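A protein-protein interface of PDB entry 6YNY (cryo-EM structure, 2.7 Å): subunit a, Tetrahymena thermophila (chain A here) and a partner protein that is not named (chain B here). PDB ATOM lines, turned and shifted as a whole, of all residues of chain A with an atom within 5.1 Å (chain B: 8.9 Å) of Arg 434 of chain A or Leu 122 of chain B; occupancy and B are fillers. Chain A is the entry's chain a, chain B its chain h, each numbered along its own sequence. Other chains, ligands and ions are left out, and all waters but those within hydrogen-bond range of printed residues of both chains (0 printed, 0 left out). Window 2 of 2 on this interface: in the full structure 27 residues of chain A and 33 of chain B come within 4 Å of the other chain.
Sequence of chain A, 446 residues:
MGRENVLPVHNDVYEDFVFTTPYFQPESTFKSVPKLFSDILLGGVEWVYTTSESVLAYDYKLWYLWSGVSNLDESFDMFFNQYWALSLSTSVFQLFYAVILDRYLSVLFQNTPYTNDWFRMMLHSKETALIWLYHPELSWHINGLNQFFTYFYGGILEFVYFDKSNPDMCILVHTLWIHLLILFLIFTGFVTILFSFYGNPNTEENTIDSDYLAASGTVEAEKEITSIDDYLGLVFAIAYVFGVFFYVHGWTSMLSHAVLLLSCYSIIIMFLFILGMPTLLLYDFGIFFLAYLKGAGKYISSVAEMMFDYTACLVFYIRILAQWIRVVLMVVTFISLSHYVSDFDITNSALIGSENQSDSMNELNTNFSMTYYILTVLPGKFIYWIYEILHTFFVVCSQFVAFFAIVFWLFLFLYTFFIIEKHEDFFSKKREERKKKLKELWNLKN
Of the printed residues of chain B, Lys 430 of chain A touches Tyr 125.
Arg 434 of chain A touches just these residues of chain B: Leu 122 (3.6 Å), Tyr 125 (3.9 Å) and Asp 126 (2.7 Å).
Lys 437 of chain A touches none of the printed residues of chain B.
Printed residues of chain B within 4 Å of Leu 438 of chain A: Asp 126 (3.7 Å).
Of the printed residues of chain A, Leu 122 of chain B touches Arg 434 (3.6 Å).
Of the printed residues of chain A, Pro 124 of chain B touches Arg 431 (2.8 Å).
Of the printed residues of chain A, Ser 127 of chain B touches Arg 431.
Of the printed residues of chain A, Thr 131 of chain B touches Arg 431.
The nearest printed residue of chain A that does not touch Leu 122 of chain B is Arg 431 of chain A (6.9 Å).
The nearest printed residue of chain A that does not touch Tyr 125 of chain B is Lys 435 of chain A (5.6 Å).
O of Pro 124 of chain B is in hydrogen-bond range of OG1 of Thr 131 of chain B (2.9 Å).
The backbone carbonyl oxygen of Leu 122 of chain B lies close to the side-chain carboxylate of Asp 126 of chain B (2.6 Å).
The side-chain hydroxyl (OG) of Ser 127 of chain B lies close to the backbone carbonyl oxygen (O) of Val 123 of chain B (3.3 Å).
Among the printed residues, merely in contact across the chains: Lys 430 of chain A with Tyr 125 of chain B (3.8 Å), Arg 431 of chain A with Tyr 125 of chain B (3.6 Å), Arg 431 of chain A with Thr 131 of chain B (3.4 Å), Arg 434 of chain A with Leu 122 of chain B (3.6 Å), Arg 434 of chain A with Tyr 125 of chain B (3.9 Å) and Leu 438 of chain A with Asp 126 of chain B (3.7 Å).
Of the 20 printed residues of chain B, 6 touch a printed residue of chain A.
Along chain B the printed residues that touch a printed residue of chain A span positions 122 to 131.
Hydrophobic or aromatic side chains of chain A within 4 Å of the printed part of chain B: Leu 438.
Among the printed residues, 9 pairs touch across the chains.
NE of Arg 434 of chain A is in salt-bridge range of OD2 of Asp 126 of chain B, 2.7 Å away.
NH1 of Arg 431 of chain A sits at hydrogen-bond distance from O of Ser 127 of chain B, at 2.8 Å.
The backbone carbonyl oxygen of Pro 124 of chain B sits at hydrogen-bond distance from the guanidinium group of Arg 431 of chain A.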
ATOM      1  N   LYS A 430     -27.975   8.410 -12.443  1.00  0.00           N
ATOM      2  CA  LYS A 430     -28.217   9.334 -13.545  1.00  0.00           C
ATOM      3  C   LYS A 430     -29.127   8.714 -14.596  1.00  0.00           C
ATOM      4  O   LYS A 430     -29.946   9.411 -15.204  1.00  0.00           O
ATOM      5  CB  LYS A 430     -26.894   9.752 -14.174  1.00  0.00           C
ATOM      6  CG  LYS A 430     -25.957  10.484 -13.246  1.00  0.00           C
ATOM      7  CD  LYS A 430     -26.331  11.932 -13.066  1.00  0.00           C
ATOM      8  CE  LYS A 430     -25.231  12.687 -12.347  1.00  0.00           C
ATOM      9  NZ  LYS A 430     -25.546  14.129 -12.192  1.00  0.00           N
ATOM     10  N   ARG A 431     -28.996   7.407 -14.828  1.00  0.00           N
ATOM     11  CA  ARG A 431     -29.877   6.732 -15.775  1.00  0.00           C
ATOM     12  C   ARG A 431     -31.322   6.762 -15.303  1.00  0.00           C
ATOM     13  O   ARG A 431     -32.247   6.862 -16.117  1.00  0.00           O
ATOM     14  CB  ARG A 431     -29.417   5.291 -15.982  1.00  0.00           C
ATOM     15  CG  ARG A 431     -28.085   5.158 -16.672  1.00  0.00           C
ATOM     16  CD  ARG A 431     -27.609   3.723 -16.691  1.00  0.00           C
ATOM     17  NE  ARG A 431     -28.527   2.845 -17.407  1.00  0.00           N
ATOM     18  CZ  ARG A 431     -28.509   2.647 -18.720  1.00  0.00           C
ATOM     19  NH1 ARG A 431     -29.388   1.830 -19.276  1.00  0.00           N
ATOM     20  NH2 ARG A 431     -27.619   3.262 -19.481  1.00  0.00           N
ATOM     21  N   GLU A 432     -31.540   6.671 -13.992  1.00  0.00           N
ATOM     22  CA  GLU A 432     -32.896   6.732 -13.463  1.00  0.00           C
ATOM     23  C   GLU A 432     -33.506   8.108 -13.683  1.00  0.00           C
ATOM     24  O   GLU A 432     -34.651   8.228 -14.131  1.00  0.00           O
ATOM     25  CB  GLU A 432     -32.887   6.382 -11.978  1.00  0.00           C
ATOM     26  CG  GLU A 432     -32.356   5.000 -11.677  1.00  0.00           C
ATOM     27  CD  GLU A 432     -32.114   4.778 -10.196  1.00  0.00           C
ATOM     28  OE1 GLU A 432     -32.452   5.677  -9.396  1.00  0.00           O
ATOM     29  OE2 GLU A 432     -31.584   3.709  -9.831  1.00  0.00           O
ATOM     30  N   GLU A 433     -32.749   9.163 -13.378  1.00  0.00           N
ATOM     31  CA  GLU A 433     -33.251  10.514 -13.592  1.00  0.00           C
ATOM     32  C   GLU A 433     -33.438  10.803 -15.073  1.00  0.00           C
ATOM     33  O   GLU A 433     -34.393  11.482 -15.466  1.00  0.00           O
ATOM     34  CB  GLU A 433     -32.291  11.524 -12.967  1.00  0.00           C
ATOM     35  CG  GLU A 433     -32.734  12.964 -13.091  1.00  0.00           C
ATOM     36  CD  GLU A 433     -31.762  13.927 -12.439  1.00  0.00           C
ATOM     37  OE1 GLU A 433     -30.673  13.480 -12.021  1.00  0.00           O
ATOM     38  OE2 GLU A 433     -32.086  15.129 -12.345  1.00  0.00           O
ATOM     39  N   ARG A 434     -32.534  10.296 -15.909  1.00  0.00           N
ATOM     40  CA  ARG A 434     -32.657  10.487 -17.348  1.00  0.00           C
ATOM     41  C   ARG A 434     -33.882   9.777 -17.908  1.00  0.00           C
ATOM     42  O   ARG A 434     -34.496  10.264 -18.863  1.00  0.00           O
ATOM     43  CB  ARG A 434     -31.392   9.992 -18.043  1.00  0.00           C
ATOM     44  CG  ARG A 434     -31.354  10.232 -19.530  1.00  0.00           C
ATOM     45  CD  ARG A 434     -31.182  11.695 -19.854  1.00  0.00           C
ATOM     46  NE  ARG A 434     -31.206  11.933 -21.291  1.00  0.00           N
ATOM     47  CZ  ARG A 434     -31.105  13.131 -21.852  1.00  0.00           C
ATOM     48  NH1 ARG A 434     -30.974  14.212 -21.095  1.00  0.00           N
ATOM     49  NH2 ARG A 434     -31.139  13.243 -23.172  1.00  0.00           N
ATOM     50  N   LYS A 435     -34.249   8.632 -17.333  1.00  0.00           N
ATOM     51  CA  LYS A 435     -35.400   7.895 -17.837  1.00  0.00           C
ATOM     52  C   LYS A 435     -36.705   8.621 -17.547  1.00  0.00           C
ATOM     53  O   LYS A 435     -37.679   8.462 -18.289  1.00  0.00           O
ATOM     54  CB  LYS A 435     -35.426   6.494 -17.236  1.00  0.00           C
ATOM     55  CG  LYS A 435     -36.504   5.608 -17.813  1.00  0.00           C
ATOM     56  CD  LYS A 435     -36.405   4.192 -17.285  1.00  0.00           C
ATOM     57  CE  LYS A 435     -37.548   3.334 -17.801  1.00  0.00           C
ATOM     58  NZ  LYS A 435     -37.670   3.402 -19.286  1.00  0.00           N
ATOM     59  N   LYS A 436     -36.748   9.410 -16.475  1.00  0.00           N
ATOM     60  CA  LYS A 436     -37.933  10.204 -16.186  1.00  0.00           C
ATOM     61  C   LYS A 436     -38.033  11.415 -17.099  1.00  0.00           C
ATOM     62  O   LYS A 436     -39.138  11.904 -17.357  1.00  0.00           O
ATOM     63  CB  LYS A 436     -37.922  10.645 -14.724  1.00  0.00           C
ATOM     64  CG  LYS A 436     -37.901   9.492 -13.736  1.00  0.00           C
ATOM     65  CD  LYS A 436     -37.670   9.969 -12.313  1.00  0.00           C
ATOM     66  CE  LYS A 436     -38.863  10.738 -11.770  1.00  0.00           C
ATOM     67  NZ  LYS A 436     -40.084   9.888 -11.673  1.00  0.00           N
ATOM     68  N   LYS A 437     -36.897  11.909 -17.594  1.00  0.00           N
ATOM     69  CA  LYS A 437     -36.913  13.045 -18.506  1.00  0.00           C
ATOM     70  C   LYS A 437     -37.444  12.652 -19.877  1.00  0.00           C
ATOM     71  O   LYS A 437     -38.042  13.482 -20.570  1.00  0.00           O
ATOM     72  CB  LYS A 437     -35.504  13.625 -18.622  1.00  0.00           C
ATOM     73  CG  LYS A 437     -35.373  14.838 -19.526  1.00  0.00           C
ATOM     74  CD  LYS A 437     -36.048  16.062 -18.939  1.00  0.00           C
ATOM     75  CE  LYS A 437     -35.829  17.282 -19.822  1.00  0.00           C
ATOM     76  NZ  LYS A 437     -36.412  18.524 -19.244  1.00  0.00           N
ATOM     77  N   LEU A 438     -37.236  11.401 -20.285  1.00  0.00           N
ATOM     78  CA  LEU A 438     -37.704  10.893 -21.566  1.00  0.00           C
ATOM     79  C   LEU A 438     -38.966  10.052 -21.429  1.00  0.00           C
ATOM     80  O   LEU A 438     -39.280   9.263 -22.325  1.00  0.00           O
ATOM     81  CB  LEU A 438     -36.607  10.073 -22.240  1.00  0.00           C
ATOM     82  CG  LEU A 438     -35.452  10.833 -22.889  1.00  0.00           C
ATOM     83  CD1 LEU A 438     -34.742  11.723 -21.891  1.00  0.00           C
ATOM     84  CD2 LEU A 438     -34.486   9.844 -23.494  1.00  0.00           C
ATOM     85  N   TYR B  88     -15.234  13.654 -15.081  1.00  0.00           N
ATOM     86  CA  TYR B  88     -16.283  13.746 -16.088  1.00  0.00           C
ATOM     87  C   TYR B  88     -16.758  15.181 -16.257  1.00  0.00           C
ATOM     88  O   TYR B  88     -17.248  15.552 -17.327  1.00  0.00           O
ATOM     89  CB  TYR B  88     -17.444  12.836 -15.692  1.00  0.00           C
ATOM     90  CG  TYR B  88     -18.307  12.348 -16.832  1.00  0.00           C
ATOM     91  CD1 TYR B  88     -19.544  12.913 -17.084  1.00  0.00           C
ATOM     92  CD2 TYR B  88     -17.889  11.307 -17.642  1.00  0.00           C
ATOM     93  CE1 TYR B  88     -20.335  12.458 -18.119  1.00  0.00           C
ATOM     94  CE2 TYR B  88     -18.670  10.850 -18.676  1.00  0.00           C
ATOM     95  CZ  TYR B  88     -19.891  11.425 -18.912  1.00  0.00           C
ATOM     96  OH  TYR B  88     -20.666  10.960 -19.947  1.00  0.00           O
ATOM     97  N   TYR B  92     -15.658  17.767 -19.735  1.00  0.00           N
ATOM     98  CA  TYR B  92     -16.644  18.509 -20.510  1.00  0.00           C
ATOM     99  C   TYR B  92     -16.234  19.967 -20.659  1.00  0.00           C
ATOM    100  O   TYR B  92     -16.252  20.521 -21.762  1.00  0.00           O
ATOM    101  CB  TYR B  92     -18.011  18.403 -19.841  1.00  0.00           C
ATOM    102  CG  TYR B  92     -19.129  19.053 -20.615  1.00  0.00           C
ATOM    103  CD1 TYR B  92     -19.900  18.320 -21.498  1.00  0.00           C
ATOM    104  CD2 TYR B  92     -19.414  20.398 -20.463  1.00  0.00           C
ATOM    105  CE1 TYR B  92     -20.918  18.906 -22.206  1.00  0.00           C
ATOM    106  CE2 TYR B  92     -20.427  20.990 -21.167  1.00  0.00           C
ATOM    107  CZ  TYR B  92     -21.178  20.241 -22.038  1.00  0.00           C
ATOM    108  OH  TYR B  92     -22.196  20.831 -22.744  1.00  0.00           O
ATOM    109  N   ILE B 114     -22.551  22.427 -28.787  1.00  0.00           N
ATOM    110  CA  ILE B 114     -22.957  21.993 -27.454  1.00  0.00           C
ATOM    111  C   ILE B 114     -23.920  20.819 -27.554  1.00  0.00           C
ATOM    112  O   ILE B 114     -23.772  19.810 -26.858  1.00  0.00           O
ATOM    113  CB  ILE B 114     -23.574  23.168 -26.677  1.00  0.00           C
ATOM    114  CG1 ILE B 114     -22.493  24.176 -26.300  1.00  0.00           C
ATOM    115  CG2 ILE B 114     -24.284  22.670 -25.443  1.00  0.00           C
ATOM    116  CD1 ILE B 114     -23.030  25.501 -25.840  1.00  0.00           C
ATOM    117  N   LEU B 115     -24.925  20.936 -28.422  1.00  0.00           N
ATOM    118  CA  LEU B 115     -25.860  19.838 -28.619  1.00  0.00           C
ATOM    119  C   LEU B 115     -25.135  18.566 -29.034  1.00  0.00           C
ATOM    120  O   LEU B 115     -25.504  17.464 -28.613  1.00  0.00           O
ATOM    121  CB  LEU B 115     -26.896  20.227 -29.667  1.00  0.00           C
ATOM    122  CG  LEU B 115     -27.741  21.449 -29.330  1.00  0.00           C
ATOM    123  CD1 LEU B 115     -28.633  21.808 -30.486  1.00  0.00           C
ATOM    124  CD2 LEU B 115     -28.563  21.205 -28.096  1.00  0.00           C
ATOM    125  N   GLY B 116     -24.098  18.698 -29.859  1.00  0.00           N
ATOM    126  CA  GLY B 116     -23.337  17.532 -30.269  1.00  0.00           C
ATOM    127  C   GLY B 116     -22.449  17.004 -29.163  1.00  0.00           C
ATOM    128  O   GLY B 116     -22.248  15.793 -29.041  1.00  0.00           O
ATOM    129  N   LEU B 117     -21.905  17.901 -28.346  1.00  0.00           N
ATOM    130  CA  LEU B 117     -21.075  17.479 -27.227  1.00  0.00           C
ATOM    131  C   LEU B 117     -21.897  16.738 -26.184  1.00  0.00           C
ATOM    132  O   LEU B 117     -21.420  15.769 -25.585  1.00  0.00           O
ATOM    133  CB  LEU B 117     -20.390  18.694 -26.614  1.00  0.00           C
ATOM    134  CG  LEU B 117     -19.322  18.432 -25.561  1.00  0.00           C
ATOM    135  CD1 LEU B 117     -18.165  17.670 -26.155  1.00  0.00           C
ATOM    136  CD2 LEU B 117     -18.853  19.739 -24.977  1.00  0.00           C
ATOM    137  N   ARG B 118     -23.136  17.175 -25.956  1.00  0.00           N
ATOM    138  CA  ARG B 118     -23.988  16.490 -24.991  1.00  0.00           C
ATOM    139  C   ARG B 118     -24.352  15.094 -25.475  1.00  0.00           C
ATOM    140  O   ARG B 118     -24.401  14.150 -24.679  1.00  0.00           O
ATOM    141  CB  ARG B 118     -25.246  17.313 -24.733  1.00  0.00           C
ATOM    142  CG  ARG B 118     -24.965  18.643 -24.081  1.00  0.00           C
ATOM    143  CD  ARG B 118     -26.219  19.471 -23.880  1.00  0.00           C
ATOM    144  NE  ARG B 118     -27.102  18.909 -22.863  1.00  0.00           N
ATOM    145  CZ  ARG B 118     -28.169  18.160 -23.113  1.00  0.00           C
ATOM    146  NH1 ARG B 118     -28.522  17.866 -24.358  1.00  0.00           N
ATOM    147  NH2 ARG B 118     -28.894  17.706 -22.105  1.00  0.00           N
ATOM    148  N   SER B 119     -24.602  14.941 -26.775  1.00  0.00           N
ATOM    149  CA  SER B 119     -24.893  13.621 -27.314  1.00  0.00           C
ATOM    150  C   SER B 119     -23.752  12.648 -27.071  1.00  0.00           C
ATOM    151  O   SER B 119     -23.980  11.436 -27.032  1.00  0.00           O
ATOM    152  CB  SER B 119     -25.179  13.720 -28.809  1.00  0.00           C
ATOM    153  OG  SER B 119     -24.014  14.072 -29.527  1.00  0.00           O
ATOM    154  N   LEU B 120     -22.534  13.157 -26.907  1.00  0.00           N
ATOM    155  CA  LEU B 120     -21.379  12.306 -26.669  1.00  0.00           C
ATOM    156  C   LEU B 120     -21.233  11.945 -25.197  1.00  0.00           C
ATOM    157  O   LEU B 120     -20.760  10.852 -24.876  1.00  0.00           O
ATOM    158  CB  LEU B 120     -20.122  13.005 -27.182  1.00  0.00           C
ATOM    159  CG  LEU B 120     -18.848  12.183 -27.299  1.00  0.00           C
ATOM    160  CD1 LEU B 120     -19.036  11.051 -28.276  1.00  0.00           C
ATOM    161  CD2 LEU B 120     -17.737  13.088 -27.748  1.00  0.00           C
ATOM    162  N   PHE B 121     -21.632  12.842 -24.298  1.00  0.00           N
ATOM    163  CA  PHE B 121     -21.570  12.582 -22.869  1.00  0.00           C
ATOM    164  C   PHE B 121     -22.800  11.861 -22.340  1.00  0.00           C
ATOM    165  O   PHE B 121     -22.733  11.272 -21.255  1.00  0.00           O
ATOM    166  CB  PHE B 121     -21.396  13.896 -22.105  1.00  0.00           C
ATOM    167  CG  PHE B 121     -20.007  14.448 -22.161  1.00  0.00           C
ATOM    168  CD1 PHE B 121     -19.201  14.447 -21.042  1.00  0.00           C
ATOM    169  CD2 PHE B 121     -19.503  14.962 -23.336  1.00  0.00           C
ATOM    170  CE1 PHE B 121     -17.928  14.949 -21.096  1.00  0.00           C
ATOM    171  CE2 PHE B 121     -18.229  15.463 -23.390  1.00  0.00           C
ATOM    172  CZ  PHE B 121     -17.442  15.456 -22.270  1.00  0.00           C
ATOM    173  N   LEU B 122     -23.910  11.893 -23.067  1.00  0.00           N
ATOM    174  CA  LEU B 122     -25.142  11.251 -22.637  1.00  0.00           C
ATOM    175  C   LEU B 122     -25.240   9.796 -23.066  1.00  0.00           C
ATOM    176  O   LEU B 122     -26.257   9.153 -22.794  1.00  0.00           O
ATOM    177  CB  LEU B 122     -26.345  12.020 -23.180  1.00  0.00           C
ATOM    178  CG  LEU B 122     -26.592  13.394 -22.566  1.00  0.00           C
ATOM    179  CD1 LEU B 122     -27.679  14.108 -23.325  1.00  0.00           C
ATOM    180  CD2 LEU B 122     -26.971  13.260 -21.114  1.00  0.00           C
ATOM    181  N   VAL B 123     -24.215   9.262 -23.725  1.00  0.00           N
ATOM    182  CA  VAL B 123     -24.259   7.867 -24.154  1.00  0.00           C
ATOM    183  C   VAL B 123     -24.431   6.923 -22.972  1.00  0.00           C
ATOM    184  O   VAL B 123     -25.261   6.004 -23.060  1.00  0.00           O
ATOM    185  CB  VAL B 123     -23.013   7.537 -24.996  1.00  0.00           C
ATOM    186  CG1 VAL B 123     -22.971   6.065 -25.335  1.00  0.00           C
ATOM    187  CG2 VAL B 123     -23.008   8.368 -26.252  1.00  0.00           C
ATOM    188  N   PRO B 124     -23.709   7.077 -21.861  1.00  0.00           N
ATOM    189  CA  PRO B 124     -23.865   6.128 -20.753  1.00  0.00           C
ATOM    190  C   PRO B 124     -25.209   6.218 -20.059  1.00  0.00           C
ATOM    191  O   PRO B 124     -25.628   5.235 -19.436  1.00  0.00           O
ATOM    192  CB  PRO B 124     -22.729   6.510 -19.797  1.00  0.00           C
ATOM    193  CG  PRO B 124     -21.849   7.412 -20.554  1.00  0.00           C
ATOM    194  CD  PRO B 124     -22.675   8.077 -21.573  1.00  0.00           C
ATOM    195  N   TYR B 125     -25.892   7.355 -20.139  1.00  0.00           N
ATOM    196  CA  TYR B 125     -27.136   7.555 -19.412  1.00  0.00           C
ATOM    197  C   TYR B 125     -28.358   7.060 -20.167  1.00  0.00           C
ATOM    198  O   TYR B 125     -29.396   6.817 -19.542  1.00  0.00           O
ATOM    199  CB  TYR B 125     -27.335   9.038 -19.089  1.00  0.00           C
ATOM    200  CG  TYR B 125     -26.218   9.684 -18.308  1.00  0.00           C
ATOM    201  CD1 TYR B 125     -25.274   8.927 -17.635  1.00  0.00           C
ATOM    202  CD2 TYR B 125     -26.116  11.062 -18.238  1.00  0.00           C
ATOM    203  CE1 TYR B 125     -24.258   9.525 -16.923  1.00  0.00           C
ATOM    204  CE2 TYR B 125     -25.106  11.667 -17.528  1.00  0.00           C
ATOM    205  CZ  TYR B 125     -24.180  10.895 -16.873  1.00  0.00           C
ATOM    206  OH  TYR B 125     -23.173  11.501 -16.166  1.00  0.00           O
ATOM    207  N   ASP B 126     -28.262   6.899 -21.482  1.00  0.00           N
ATOM    208  CA  ASP B 126     -29.411   6.579 -22.312  1.00  0.00           C
ATOM    209  C   ASP B 126     -29.264   5.282 -23.089  1.00  0.00           C
ATOM    210  O   ASP B 126     -30.201   4.894 -23.796  1.00  0.00           O
ATOM    211  CB  ASP B 126     -29.672   7.721 -23.300  1.00  0.00           C
ATOM    212  CG  ASP B 126     -29.784   9.068 -22.621  1.00  0.00           C
ATOM    213  OD1 ASP B 126     -28.744   9.600 -22.184  1.00  0.00           O
ATOM    214  OD2 ASP B 126     -30.911   9.597 -22.529  1.00  0.00           O
ATOM    215  N   SER B 127     -28.131   4.603 -22.985  1.00  0.00           N
ATOM    216  CA  SER B 127     -27.899   3.402 -23.764  1.00  0.00           C
ATOM    217  C   SER B 127     -28.666   2.216 -23.189  1.00  0.00           C
ATOM    218  O   SER B 127     -29.006   2.173 -22.004  1.00  0.00           O
ATOM    219  CB  SER B 127     -26.410   3.078 -23.806  1.00  0.00           C
ATOM    220  OG  SER B 127     -25.918   2.805 -22.509  1.00  0.00           O
ATOM    221  N   GLN B 128     -28.940   1.243 -24.058  1.00  0.00           N
ATOM    222  CA  GLN B 128     -29.511  -0.016 -23.598  1.00  0.00           C
ATOM    223  C   GLN B 128     -28.537  -0.748 -22.689  1.00  0.00           C
ATOM    224  O   GLN B 128     -28.946  -1.419 -21.735  1.00  0.00           O
ATOM    225  CB  GLN B 128     -29.876  -0.896 -24.789  1.00  0.00           C
ATOM    226  CG  GLN B 128     -30.717  -0.223 -25.839  1.00  0.00           C
ATOM    227  CD  GLN B 128     -31.014  -1.140 -27.002  1.00  0.00           C
ATOM    228  OE1 GLN B 128     -31.245  -2.334 -26.821  1.00  0.00           O
ATOM    229  NE2 GLN B 128     -30.991  -0.592 -28.207  1.00  0.00           N
ATOM    230  N   THR B 131     -24.776   0.504 -18.124  1.00  0.00           N
ATOM    231  CA  THR B 131     -23.447   1.035 -17.871  1.00  0.00           C
ATOM    232  C   THR B 131     -23.072   0.972 -16.400  1.00  0.00           C
ATOM    233  O   THR B 131     -21.883   1.037 -16.073  1.00  0.00           O
ATOM    234  CB  THR B 131     -23.360   2.470 -18.379  1.00  0.00           C
ATOM    235  OG1 THR B 131     -24.379   3.262 -17.760  1.00  0.00           O
ATOM    236  CG2 THR B 131     -23.540   2.501 -19.875  1.00  0.00           C
ATOM    237  N   PHE B 142     -15.523   5.204 -19.348  1.00  0.00           N
ATOM    238  CA  PHE B 142     -15.952   6.277 -20.237  1.00  0.00           C
ATOM    239  C   PHE B 142     -15.128   7.539 -20.028  1.00  0.00           C
ATOM    240  O   PHE B 142     -14.804   8.241 -20.992  1.00  0.00           O
ATOM    241  CB  PHE B 142     -17.434   6.567 -20.023  1.00  0.00           C
ATOM    242  CG  PHE B 142     -18.342   5.649 -20.774  1.00  0.00           C
ATOM    243  CD1 PHE B 142     -18.860   6.024 -21.995  1.00  0.00           C
ATOM    244  CD2 PHE B 142     -18.668   4.409 -20.269  1.00  0.00           C
ATOM    245  CE1 PHE B 142     -19.692   5.185 -22.689  1.00  0.00           C
ATOM    246  CE2 PHE B 142     -19.497   3.567 -20.961  1.00  0.00           C
ATOM    247  CZ  PHE B 142     -20.010   3.956 -22.173  1.00  0.00           C
ATOM    248  N   LEU B 146     -13.132   9.594 -22.889  1.00  0.00           N
ATOM    249  CA  LEU B 146     -13.294  10.999 -23.234  1.00  0.00           C
ATOM    250  C   LEU B 146     -11.981  11.757 -23.129  1.00  0.00           C
ATOM    251  O   LEU B 146     -11.762  12.724 -23.865  1.00  0.00           O
ATOM    252  CB  LEU B 146     -14.341  11.632 -22.324  1.00  0.00           C
ATOM    253  CG  LEU B 146     -15.746  11.056 -22.449  1.00  0.00           C
ATOM    254  CD1 LEU B 146     -16.594  11.476 -21.274  1.00  0.00           C
ATOM    255  CD2 LEU B 146     -16.376  11.504 -23.738  1.00  0.00           C
